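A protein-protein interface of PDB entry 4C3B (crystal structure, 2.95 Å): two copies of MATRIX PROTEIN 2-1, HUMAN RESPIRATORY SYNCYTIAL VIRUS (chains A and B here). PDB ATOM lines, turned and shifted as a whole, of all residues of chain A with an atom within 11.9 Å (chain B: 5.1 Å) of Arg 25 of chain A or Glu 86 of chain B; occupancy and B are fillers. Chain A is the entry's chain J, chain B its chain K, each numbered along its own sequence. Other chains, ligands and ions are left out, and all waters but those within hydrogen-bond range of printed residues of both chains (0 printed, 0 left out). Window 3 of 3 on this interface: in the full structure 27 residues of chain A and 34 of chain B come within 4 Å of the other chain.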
ATOM      1  N   ARG A   9     -38.225  14.984  14.724  1.00  0.00           N
ATOM      2  CA  ARG A   9     -37.302  13.847  14.553  1.00  0.00           C
ATOM      3  C   ARG A   9     -37.922  12.512  14.978  1.00  0.00           C
ATOM      4  O   ARG A   9     -38.455  12.395  16.066  1.00  0.00           O
ATOM      5  CB  ARG A   9     -36.074  14.003  15.423  1.00  0.00           C
ATOM      6  CG  ARG A   9     -35.094  15.072  15.016  1.00  0.00           C
ATOM      7  CD  ARG A   9     -33.739  14.745  15.636  1.00  0.00           C
ATOM      8  NE  ARG A   9     -32.727  15.790  15.470  1.00  0.00           N
ATOM      9  CZ  ARG A   9     -32.141  16.119  14.316  1.00  0.00           C
ATOM     10  NH1 ARG A   9     -32.472  15.512  13.181  1.00  0.00           N
ATOM     11  NH2 ARG A   9     -31.220  17.079  14.292  1.00  0.00           N
ATOM     12  N   ASN A  10     -37.818  11.499  14.125  1.00  0.00           N
ATOM     13  CA  ASN A  10     -38.219  10.156  14.511  1.00  0.00           C
ATOM     14  C   ASN A  10     -37.260   9.434  15.470  1.00  0.00           C
ATOM     15  O   ASN A  10     -36.071   9.708  15.525  1.00  0.00           O
ATOM     16  CB  ASN A  10     -38.393   9.268  13.281  1.00  0.00           C
ATOM     17  CG  ASN A  10     -39.570   9.672  12.431  1.00  0.00           C
ATOM     18  OD1 ASN A  10     -40.650   9.977  12.939  1.00  0.00           O
ATOM     19  ND2 ASN A  10     -39.360   9.702  11.134  1.00  0.00           N
ATOM     20  N   CYS A  12     -34.677   6.959  16.976  1.00  0.00           N
ATOM     21  CA  CYS A  12     -33.608   6.087  16.547  1.00  0.00           C
ATOM     22  C   CYS A  12     -33.921   4.616  16.787  1.00  0.00           C
ATOM     23  O   CYS A  12     -34.071   4.183  17.925  1.00  0.00           O
ATOM     24  CB  CYS A  12     -32.352   6.414  17.313  1.00  0.00           C
ATOM     25  SG  CYS A  12     -30.950   5.320  16.990  1.00  0.00           S
ATOM     26  N   LYS A  13     -34.023   3.845  15.707  1.00  0.00           N
ATOM     27  CA  LYS A  13     -34.365   2.433  15.792  1.00  0.00           C
ATOM     28  C   LYS A  13     -33.286   1.641  16.505  1.00  0.00           C
ATOM     29  O   LYS A  13     -33.563   0.599  17.033  1.00  0.00           O
ATOM     30  CB  LYS A  13     -34.664   1.854  14.407  1.00  0.00           C
ATOM     31  CG  LYS A  13     -36.006   2.336  13.834  1.00  0.00           C
ATOM     32  CD  LYS A  13     -36.247   1.975  12.360  1.00  0.00           C
ATOM     33  CE  LYS A  13     -36.392   0.460  12.096  1.00  0.00           C
ATOM     34  NZ  LYS A  13     -37.409  -0.276  12.921  1.00  0.00           N
ATOM     35  N   PHE A  14     -32.058   2.116  16.537  1.00  0.00           N
ATOM     36  CA  PHE A  14     -31.037   1.410  17.299  1.00  0.00           C
ATOM     37  C   PHE A  14     -31.325   1.536  18.782  1.00  0.00           C
ATOM     38  O   PHE A  14     -31.084   0.583  19.513  1.00  0.00           O
ATOM     39  CB  PHE A  14     -29.620   1.967  17.022  1.00  0.00           C
ATOM     40  CG  PHE A  14     -29.070   1.563  15.703  1.00  0.00           C
ATOM     41  CD1 PHE A  14     -29.401   2.300  14.555  1.00  0.00           C
ATOM     42  CD2 PHE A  14     -28.269   0.443  15.593  1.00  0.00           C
ATOM     43  CE1 PHE A  14     -28.934   1.910  13.331  1.00  0.00           C
ATOM     44  CE2 PHE A  14     -27.788   0.057  14.375  1.00  0.00           C
ATOM     45  CZ  PHE A  14     -28.115   0.796  13.242  1.00  0.00           C
ATOM     46  N   HIS A  19     -29.270   0.700  23.060  1.00  0.00           N
ATOM     47  CA  HIS A  19     -28.430   1.875  23.039  1.00  0.00           C
ATOM     48  C   HIS A  19     -27.838   2.123  21.664  1.00  0.00           C
ATOM     49  O   HIS A  19     -26.996   1.365  21.225  1.00  0.00           O
ATOM     50  CB  HIS A  19     -27.359   1.731  24.103  1.00  0.00           C
ATOM     51  CG  HIS A  19     -27.933   1.626  25.489  1.00  0.00           C
ATOM     52  ND1 HIS A  19     -28.610   2.672  26.102  1.00  0.00           N
ATOM     53  CD2 HIS A  19     -27.946   0.600  26.375  1.00  0.00           C
ATOM     54  CE1 HIS A  19     -28.998   2.294  27.308  1.00  0.00           C
ATOM     55  NE2 HIS A  19     -28.605   1.045  27.499  1.00  0.00           N
ATOM     56  N   CYS A  20     -28.336   3.146  20.965  1.00  0.00           N
ATOM     57  CA  CYS A  20     -27.713   3.625  19.709  1.00  0.00           C
ATOM     58  C   CYS A  20     -26.184   3.799  19.836  1.00  0.00           C
ATOM     59  O   CYS A  20     -25.748   4.325  20.800  1.00  0.00           O
ATOM     60  CB  CYS A  20     -28.353   4.928  19.255  1.00  0.00           C
ATOM     61  SG  CYS A  20     -27.559   5.621  17.807  1.00  0.00           S
ATOM     62  N   LEU A  21     -25.385   3.298  18.895  1.00  0.00           N
ATOM     63  CA  LEU A  21     -23.935   3.266  19.100  1.00  0.00           C
ATOM     64  C   LEU A  21     -23.215   4.132  18.078  1.00  0.00           C
ATOM     65  O   LEU A  21     -21.983   4.034  17.919  1.00  0.00           O
ATOM     66  CB  LEU A  21     -23.399   1.824  19.021  1.00  0.00           C
ATOM     67  CG  LEU A  21     -23.807   0.849  20.108  1.00  0.00           C
ATOM     68  CD1 LEU A  21     -23.130  -0.495  19.958  1.00  0.00           C
ATOM     69  CD2 LEU A  21     -23.442   1.452  21.447  1.00  0.00           C
ATOM     70  N   ASN A  22     -23.970   5.007  17.436  1.00  0.00           N
ATOM     71  CA  ASN A  22     -23.423   5.827  16.397  1.00  0.00           C
ATOM     72  C   ASN A  22     -22.980   7.229  16.810  1.00  0.00           C
ATOM     73  O   ASN A  22     -22.682   8.038  15.938  1.00  0.00           O
ATOM     74  CB  ASN A  22     -24.456   5.937  15.293  1.00  0.00           C
ATOM     75  CG  ASN A  22     -24.661   4.620  14.597  1.00  0.00           C
ATOM     76  OD1 ASN A  22     -23.682   3.963  14.242  1.00  0.00           O
ATOM     77  ND2 ASN A  22     -25.903   4.244  14.353  1.00  0.00           N
ATOM     78  N   GLY A  23     -22.888   7.518  18.107  1.00  0.00           N
ATOM     79  CA  GLY A  23     -22.507   8.856  18.570  1.00  0.00           C
ATOM     80  C   GLY A  23     -23.212  10.009  17.865  1.00  0.00           C
ATOM     81  O   GLY A  23     -24.375   9.866  17.432  1.00  0.00           O
ATOM     82  N   LYS A  24     -22.464  11.118  17.685  1.00  0.00           N
ATOM     83  CA  LYS A  24     -22.984  12.356  17.116  1.00  0.00           C
ATOM     84  C   LYS A  24     -23.483  12.210  15.669  1.00  0.00           C
ATOM     85  O   LYS A  24     -24.355  12.964  15.213  1.00  0.00           O
ATOM     86  CB  LYS A  24     -21.919  13.443  17.159  1.00  0.00           C
ATOM     87  CG  LYS A  24     -21.985  14.430  18.316  1.00  0.00           C
ATOM     88  CD  LYS A  24     -21.172  15.709  18.001  1.00  0.00           C
ATOM     89  CE  LYS A  24     -21.616  16.965  18.769  1.00  0.00           C
ATOM     90  NZ  LYS A  24     -20.948  17.185  20.100  1.00  0.00           N
ATOM     91  N   ARG A  25     -22.945  11.239  14.944  1.00  0.00           N
ATOM     92  CA  ARG A  25     -23.328  11.031  13.550  1.00  0.00           C
ATOM     93  C   ARG A  25     -24.823  10.827  13.383  1.00  0.00           C
ATOM     94  O   ARG A  25     -25.388  11.248  12.385  1.00  0.00           O
ATOM     95  CB  ARG A  25     -22.559   9.839  12.947  1.00  0.00           C
ATOM     96  CG  ARG A  25     -21.052  10.077  12.950  1.00  0.00           C
ATOM     97  CD  ARG A  25     -20.230   8.993  13.651  1.00  0.00           C
ATOM     98  NE  ARG A  25     -19.584   8.089  12.702  1.00  0.00           N
ATOM     99  CZ  ARG A  25     -19.959   6.835  12.452  1.00  0.00           C
ATOM    100  NH1 ARG A  25     -20.998   6.282  13.085  1.00  0.00           N
ATOM    101  NH2 ARG A  25     -19.287   6.130  11.552  1.00  0.00           N
ATOM    102  N   CYS A  26     -25.425  10.116  14.328  1.00  0.00           N
ATOM    103  CA  CYS A  26     -26.802   9.674  14.204  1.00  0.00           C
ATOM    104  C   CYS A  26     -27.751  10.828  14.381  1.00  0.00           C
ATOM    105  O   CYS A  26     -27.751  11.452  15.424  1.00  0.00           O
ATOM    106  CB  CYS A  26     -27.107   8.588  15.253  1.00  0.00           C
ATOM    107  SG  CYS A  26     -28.798   7.949  15.149  1.00  0.00           S
ATOM    108  N   HIS A  27     -28.627  11.025  13.406  1.00  0.00           N
ATOM    109  CA  HIS A  27     -29.496  12.183  13.397  1.00  0.00           C
ATOM    110  C   HIS A  27     -30.934  11.862  13.754  1.00  0.00           C
ATOM    111  O   HIS A  27     -31.831  12.674  13.586  1.00  0.00           O
ATOM    112  CB  HIS A  27     -29.375  12.903  12.051  1.00  0.00           C
ATOM    113  CG  HIS A  27     -28.164  13.785  11.971  1.00  0.00           C
ATOM    114  ND1 HIS A  27     -27.268  13.751  10.922  1.00  0.00           N
ATOM    115  CD2 HIS A  27     -27.671  14.692  12.854  1.00  0.00           C
ATOM    116  CE1 HIS A  27     -26.295  14.617  11.145  1.00  0.00           C
ATOM    117  NE2 HIS A  27     -26.514  15.199  12.312  1.00  0.00           N
ATOM    118  N   PHE A  28     -31.148  10.680  14.312  1.00  0.00           N
ATOM    119  CA  PHE A  28     -32.456  10.312  14.850  1.00  0.00           C
ATOM    120  C   PHE A  28     -32.588  10.741  16.317  1.00  0.00           C
ATOM    121  O   PHE A  28     -31.580  10.888  17.016  1.00  0.00           O
ATOM    122  CB  PHE A  28     -32.643   8.799  14.719  1.00  0.00           C
ATOM    123  CG  PHE A  28     -32.911   8.380  13.323  1.00  0.00           C
ATOM    124  CD1 PHE A  28     -34.166   8.583  12.776  1.00  0.00           C
ATOM    125  CD2 PHE A  28     -31.901   7.864  12.532  1.00  0.00           C
ATOM    126  CE1 PHE A  28     -34.429   8.247  11.472  1.00  0.00           C
ATOM    127  CE2 PHE A  28     -32.153   7.538  11.225  1.00  0.00           C
ATOM    128  CZ  PHE A  28     -33.425   7.723  10.694  1.00  0.00           C
ATOM    129  N   SER A  29     -33.822  10.892  16.794  1.00  0.00           N
ATOM    130  CA  SER A  29     -34.017  11.251  18.184  1.00  0.00           C
ATOM    131  C   SER A  29     -33.507  10.209  19.172  1.00  0.00           C
ATOM    132  O   SER A  29     -33.887   9.063  19.069  1.00  0.00           O
ATOM    133  CB  SER A  29     -35.483  11.472  18.479  1.00  0.00           C
ATOM    134  OG  SER A  29     -35.572  11.825  19.865  1.00  0.00           O
ATOM    135  N   HIS A  30     -32.742  10.618  20.166  1.00  0.00           N
ATOM    136  CA  HIS A  30     -32.509   9.777  21.326  1.00  0.00           C
ATOM    137  C   HIS A  30     -33.073  10.375  22.619  1.00  0.00           C
ATOM    138  O   HIS A  30     -32.627  10.058  23.739  1.00  0.00           O
ATOM    139  CB  HIS A  30     -31.021   9.500  21.506  1.00  0.00           C
ATOM    140  CG  HIS A  30     -30.332   9.104  20.245  1.00  0.00           C
ATOM    141  ND1 HIS A  30     -29.902  10.023  19.323  1.00  0.00           N
ATOM    142  CD2 HIS A  30     -30.010   7.892  19.747  1.00  0.00           C
ATOM    143  CE1 HIS A  30     -29.319   9.397  18.321  1.00  0.00           C
ATOM    144  NE2 HIS A  30     -29.381   8.103  18.548  1.00  0.00           N
ATOM    145  N   ALA B  78     -17.720  10.941  20.607  1.00  0.00           N
ATOM    146  CA  ALA B  78     -18.573  11.497  19.529  1.00  0.00           C
ATOM    147  C   ALA B  78     -18.668  10.541  18.349  1.00  0.00           C
ATOM    148  O   ALA B  78     -19.597  10.645  17.512  1.00  0.00           O
ATOM    149  CB  ALA B  78     -18.047  12.851  19.054  1.00  0.00           C
ATOM    150  N   LEU B  79     -17.676   9.650  18.268  1.00  0.00           N
ATOM    151  CA  LEU B  79     -17.639   8.656  17.214  1.00  0.00           C
ATOM    152  C   LEU B  79     -18.675   7.567  17.433  1.00  0.00           C
ATOM    153  O   LEU B  79     -19.373   7.121  16.499  1.00  0.00           O
ATOM    154  CB  LEU B  79     -16.253   8.023  17.162  1.00  0.00           C
ATOM    155  CG  LEU B  79     -15.160   8.741  16.360  1.00  0.00           C
ATOM    156  CD1 LEU B  79     -13.843   8.000  16.568  1.00  0.00           C
ATOM    157  CD2 LEU B  79     -15.500   8.809  14.871  1.00  0.00           C
ATOM    158  N   VAL B  81     -19.231   3.675  19.443  1.00  0.00           N
ATOM    159  CA  VAL B  81     -18.574   2.396  19.276  1.00  0.00           C
ATOM    160  C   VAL B  81     -18.518   2.009  17.790  1.00  0.00           C
ATOM    161  O   VAL B  81     -17.502   1.527  17.299  1.00  0.00           O
ATOM    162  CB  VAL B  81     -19.317   1.331  20.078  1.00  0.00           C
ATOM    163  CG1 VAL B  81     -18.792  -0.049  19.757  1.00  0.00           C
ATOM    164  CG2 VAL B  81     -19.138   1.628  21.552  1.00  0.00           C
ATOM    165  N   VAL B  82     -19.593   2.239  17.067  1.00  0.00           N
ATOM    166  CA  VAL B  82     -19.558   2.043  15.644  1.00  0.00           C
ATOM    167  C   VAL B  82     -18.474   2.912  14.965  1.00  0.00           C
ATOM    168  O   VAL B  82     -17.703   2.431  14.129  1.00  0.00           O
ATOM    169  CB  VAL B  82     -20.931   2.370  15.050  1.00  0.00           C
ATOM    170  CG1 VAL B  82     -20.876   2.399  13.524  1.00  0.00           C
ATOM    171  CG2 VAL B  82     -21.954   1.343  15.514  1.00  0.00           C
ATOM    172  N   GLY B  83     -18.469   4.206  15.283  1.00  0.00           N
ATOM    173  CA  GLY B  83     -17.520   5.143  14.715  1.00  0.00           C
ATOM    174  C   GLY B  83     -16.138   4.655  15.017  1.00  0.00           C
ATOM    175  O   GLY B  83     -15.308   4.555  14.134  1.00  0.00           O
ATOM    176  N   VAL B  84     -15.862   4.328  16.261  1.00  0.00           N
ATOM    177  CA  VAL B  84     -14.557   3.807  16.580  1.00  0.00           C
ATOM    178  C   VAL B  84     -14.251   2.620  15.697  1.00  0.00           C
ATOM    179  O   VAL B  84     -13.167   2.528  15.172  1.00  0.00           O
ATOM    180  CB  VAL B  84     -14.454   3.353  18.042  1.00  0.00           C
ATOM    181  CG1 VAL B  84     -13.246   2.447  18.262  1.00  0.00           C
ATOM    182  CG2 VAL B  84     -14.368   4.551  18.937  1.00  0.00           C
ATOM    183  N   LEU B  85     -15.176   1.678  15.579  1.00  0.00           N
ATOM    184  CA  LEU B  85     -14.856   0.437  14.907  1.00  0.00           C
ATOM    185  C   LEU B  85     -14.656   0.669  13.405  1.00  0.00           C
ATOM    186  O   LEU B  85     -13.702   0.144  12.826  1.00  0.00           O
ATOM    187  CB  LEU B  85     -15.944  -0.603  15.164  1.00  0.00           C
ATOM    188  CG  LEU B  85     -16.014  -1.185  16.586  1.00  0.00           C
ATOM    189  CD1 LEU B  85     -17.285  -2.009  16.703  1.00  0.00           C
ATOM    190  CD2 LEU B  85     -14.814  -2.045  16.957  1.00  0.00           C
ATOM    191  N   GLU B  86     -15.547   1.444  12.784  1.00  0.00           N
ATOM    192  CA  GLU B  86     -15.418   1.782  11.376  1.00  0.00           C
ATOM    193  C   GLU B  86     -14.112   2.555  11.099  1.00  0.00           C
ATOM    194  O   GLU B  86     -13.451   2.313  10.085  1.00  0.00           O
ATOM    195  CB  GLU B  86     -16.612   2.603  10.924  1.00  0.00           C
ATOM    196  CG  GLU B  86     -17.878   1.797  10.829  1.00  0.00           C
ATOM    197  CD  GLU B  86     -19.075   2.613  10.408  1.00  0.00           C
ATOM    198  OE1 GLU B  86     -18.949   3.847  10.292  1.00  0.00           O
ATOM    199  OE2 GLU B  86     -20.155   2.026  10.188  1.00  0.00           O
ATOM    200  N   SER B  87     -13.729   3.444  12.018  1.00  0.00           N
ATOM    201  CA  SER B  87     -12.454   4.127  11.962  1.00  0.00           C
ATOM    202  C   SER B  87     -11.297   3.133  12.070  1.00  0.00           C
ATOM    203  O   SER B  87     -10.383   3.175  11.283  1.00  0.00           O
ATOM    204  CB  SER B  87     -12.329   5.172  13.072  1.00  0.00           C
ATOM    205  OG  SER B  87     -13.249   6.250  12.907  1.00  0.00           O
ATOM    206  N   TYR B  88     -11.332   2.197  12.996  1.00  0.00           N
ATOM    207  CA  TYR B  88     -10.226   1.247  13.077  1.00  0.00           C
ATOM    208  C   TYR B  88     -10.040   0.459  11.797  1.00  0.00           C
ATOM    209  O   TYR B  88      -8.948  -0.018  11.513  1.00  0.00           O
ATOM    210  CB  TYR B  88     -10.433   0.249  14.192  1.00  0.00           C
ATOM    211  CG  TYR B  88      -9.414  -0.856  14.189  1.00  0.00           C
ATOM    212  CD1 TYR B  88      -8.178  -0.669  14.727  1.00  0.00           C
ATOM    213  CD2 TYR B  88      -9.712  -2.112  13.671  1.00  0.00           C
ATOM    214  CE1 TYR B  88      -7.245  -1.691  14.752  1.00  0.00           C
ATOM    215  CE2 TYR B  88      -8.790  -3.154  13.699  1.00  0.00           C
ATOM    216  CZ  TYR B  88      -7.557  -2.937  14.232  1.00  0.00           C
ATOM    217  OH  TYR B  88      -6.601  -3.926  14.264  1.00  0.00           O
ATOM    218  N   ILE B  89     -11.137   0.234  11.088  1.00  0.00           N
ATOM    219  CA  ILE B  89     -11.109  -0.561   9.873  1.00  0.00           C
ATOM    220  C   ILE B  89     -10.394   0.218   8.791  1.00  0.00           C
ATOM    221  O   ILE B  89      -9.513  -0.334   8.127  1.00  0.00           O
ATOM    222  CB  ILE B  89     -12.540  -0.939   9.424  1.00  0.00           C
ATOM    223  CG1 ILE B  89     -12.995  -2.185  10.169  1.00  0.00           C
ATOM    224  CG2 ILE B  89     -12.621  -1.152   7.917  1.00  0.00           C
ATOM    225  CD1 ILE B  89     -14.478  -2.403  10.049  1.00  0.00           C
ATOM    226  N   GLY B  90     -10.804   1.477   8.611  1.00  0.00           N
ATOM    227  CA  GLY B  90     -10.159   2.380   7.663  1.00  0.00           C
ATOM    228  C   GLY B  90      -8.867   3.043   8.153  1.00  0.00           C
ATOM    229  O   GLY B  90      -8.355   3.955   7.521  1.00  0.00           O
ATOM    230  N   LEU B 170     -20.717  -5.587  12.460  1.00  0.00           N
ATOM    231  CA  LEU B 170     -21.365  -4.327  12.191  1.00  0.00           C
ATOM    232  C   LEU B 170     -22.503  -4.456  11.187  1.00  0.00           C
ATOM    233  O   LEU B 170     -23.491  -3.724  11.268  1.00  0.00           O
ATOM    234  CB  LEU B 170     -20.355  -3.293  11.681  1.00  0.00           C
ATOM    235  CG  LEU B 170     -19.352  -2.722  12.692  1.00  0.00           C
ATOM    236  CD1 LEU B 170     -18.297  -1.911  11.979  1.00  0.00           C
ATOM    237  CD2 LEU B 170     -20.090  -1.862  13.700  1.00  0.00           C
ATOM    238  N   LYS B 174     -26.389  -3.609  11.822  1.00  0.00           N
ATOM    239  CA  LYS B 174     -27.207  -2.698  11.020  1.00  0.00           C
ATOM    240  C   LYS B 174     -28.427  -3.425  10.497  1.00  0.00           C
ATOM    241  O   LYS B 174     -29.527  -2.862  10.481  1.00  0.00           O
ATOM    242  CB  LYS B 174     -26.432  -2.076   9.867  1.00  0.00           C
ATOM    243  CG  LYS B 174     -25.255  -1.250  10.366  1.00  0.00           C
ATOM    244  CD  LYS B 174     -24.291  -0.861   9.268  1.00  0.00           C
ATOM    245  CE  LYS B 174     -24.992   0.021   8.236  1.00  0.00           C
ATOM    246  NZ  LYS B 174     -23.994   0.823   7.478  1.00  0.00           N
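N of Asn 22 of chain A lies close to SG of Cys 20 of chain A (3.7 Å).
The backbone carbonyl oxygen (O) of Arg 25 of chain A sits at hydrogen-bond distance from a ring nitrogen (ND1) of His 27 of chain A.
The backbone carbonyl oxygen (O) of Gly 83 of chain B is in hydrogen-bond range of the side-chain hydroxyl (OG) of Ser 87 of chain B, at 2.9 Å.
No position is printed for both chains.
Of the 11 pairs that touch across the chains among the printed residues, none has its exchanged pair printed and touching as well.
Among the printed residues, pairs that only touch across the chains: Asn 22 of chain A with Val 82 of chain B, Gly 23 of chain A with Ala 78 of chain B, Gly 23 of chain A with Leu 79 of chain B, Arg 25 of chain A with Leu 79 of chain B, Arg 25 of chain A with Val 82 of chain B and Arg 25 of chain A with Gly 83 of chain B.
Of the printed residues of chain A, Glu 86 of chain B touches Arg 25 (2.6 Å).
Of chain A, only Gly 23 (3.6 Å) and Lys 24 (2.9 Å) come within 4 Å of Ala 78 of chain B.
Of chain A, only Asn 22, Gly 23 and Arg 25 come within 4 Å of Leu 79 of chain B.
Of chain A, only Arg 25 (3.7 Å) comes within 4 Å of Gly 83 of chain B.
No residue of chain A comes within 4 Å of Val 84 of chain B.
No residue of chain A comes within 4 Å of Leu 85 of chain B.
No residue of chain A comes within 4 Å of Gly 90 of chain B.
Of the printed residues of chain B, Asn 22 of chain A touches Leu 79 (3.5 Å) and Val 82 (3.3 Å).
Of the printed residues of chain A, Val 81 of chain B touches Leu 21 (3.2 Å).
Printed residues of chain B within 4 Å of Gly 23 of chain A: Ala 78 and Leu 79.
Printed residues of chain B within 4 Å of Leu 21 of chain A: Val 81 (3.2 Å) and Val 82 (3.1 Å).
The nearest residue of chain B that does not touch Arg 25 of chain A is Ala 78 of chain B (4.2 Å).
N of Val 81 of chain B is in hydrogen-bond range of O of Leu 21 of chain A (3.2 Å).
The backbone NH of Val 82 of chain B lies within hydrogen-bond range of the backbone carbonyl oxygen of Leu 21 of chain A, at 3.1 Å.
The backbone carbonyl oxygen (O) of Ala 78 of chain B is in hydrogen-bond range of the backbone NH (N) of Lys 24 of chain A.
OE1 of Glu 86 of chain B lies within salt-bridge range of NH2 of Arg 25 of chain A, 2.6 Å away.
The backbone carbonyl oxygen (O) of Leu 79 of chain B sits close to the backbone carbonyl oxygen (O) of Asn 22 of chain A, at 3.5 Å.
Printed residues of chain B that touch a printed residue of chain A: Ala 78, Leu 79, Val 81, Val 82, Gly 83 and Glu 86.
Printed residues of chain A that touch a printed residue of chain B: Leu 21, Asn 22, Gly 23, Lys 24 and Arg 25.
Hydrophobic or aromatic side chains of chain A that line the printed part of chain B: Leu 21.
Along chain A the printed residues that touch a printed residue of chain B span positions 21 to 25.
Among the printed residues, Asp or Glu carboxylates within 4 Å of a Lys or Arg side-chain nitrogen of the other chain: Arg 25 of chain A with Glu 86 of chain B (2.6 Å).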
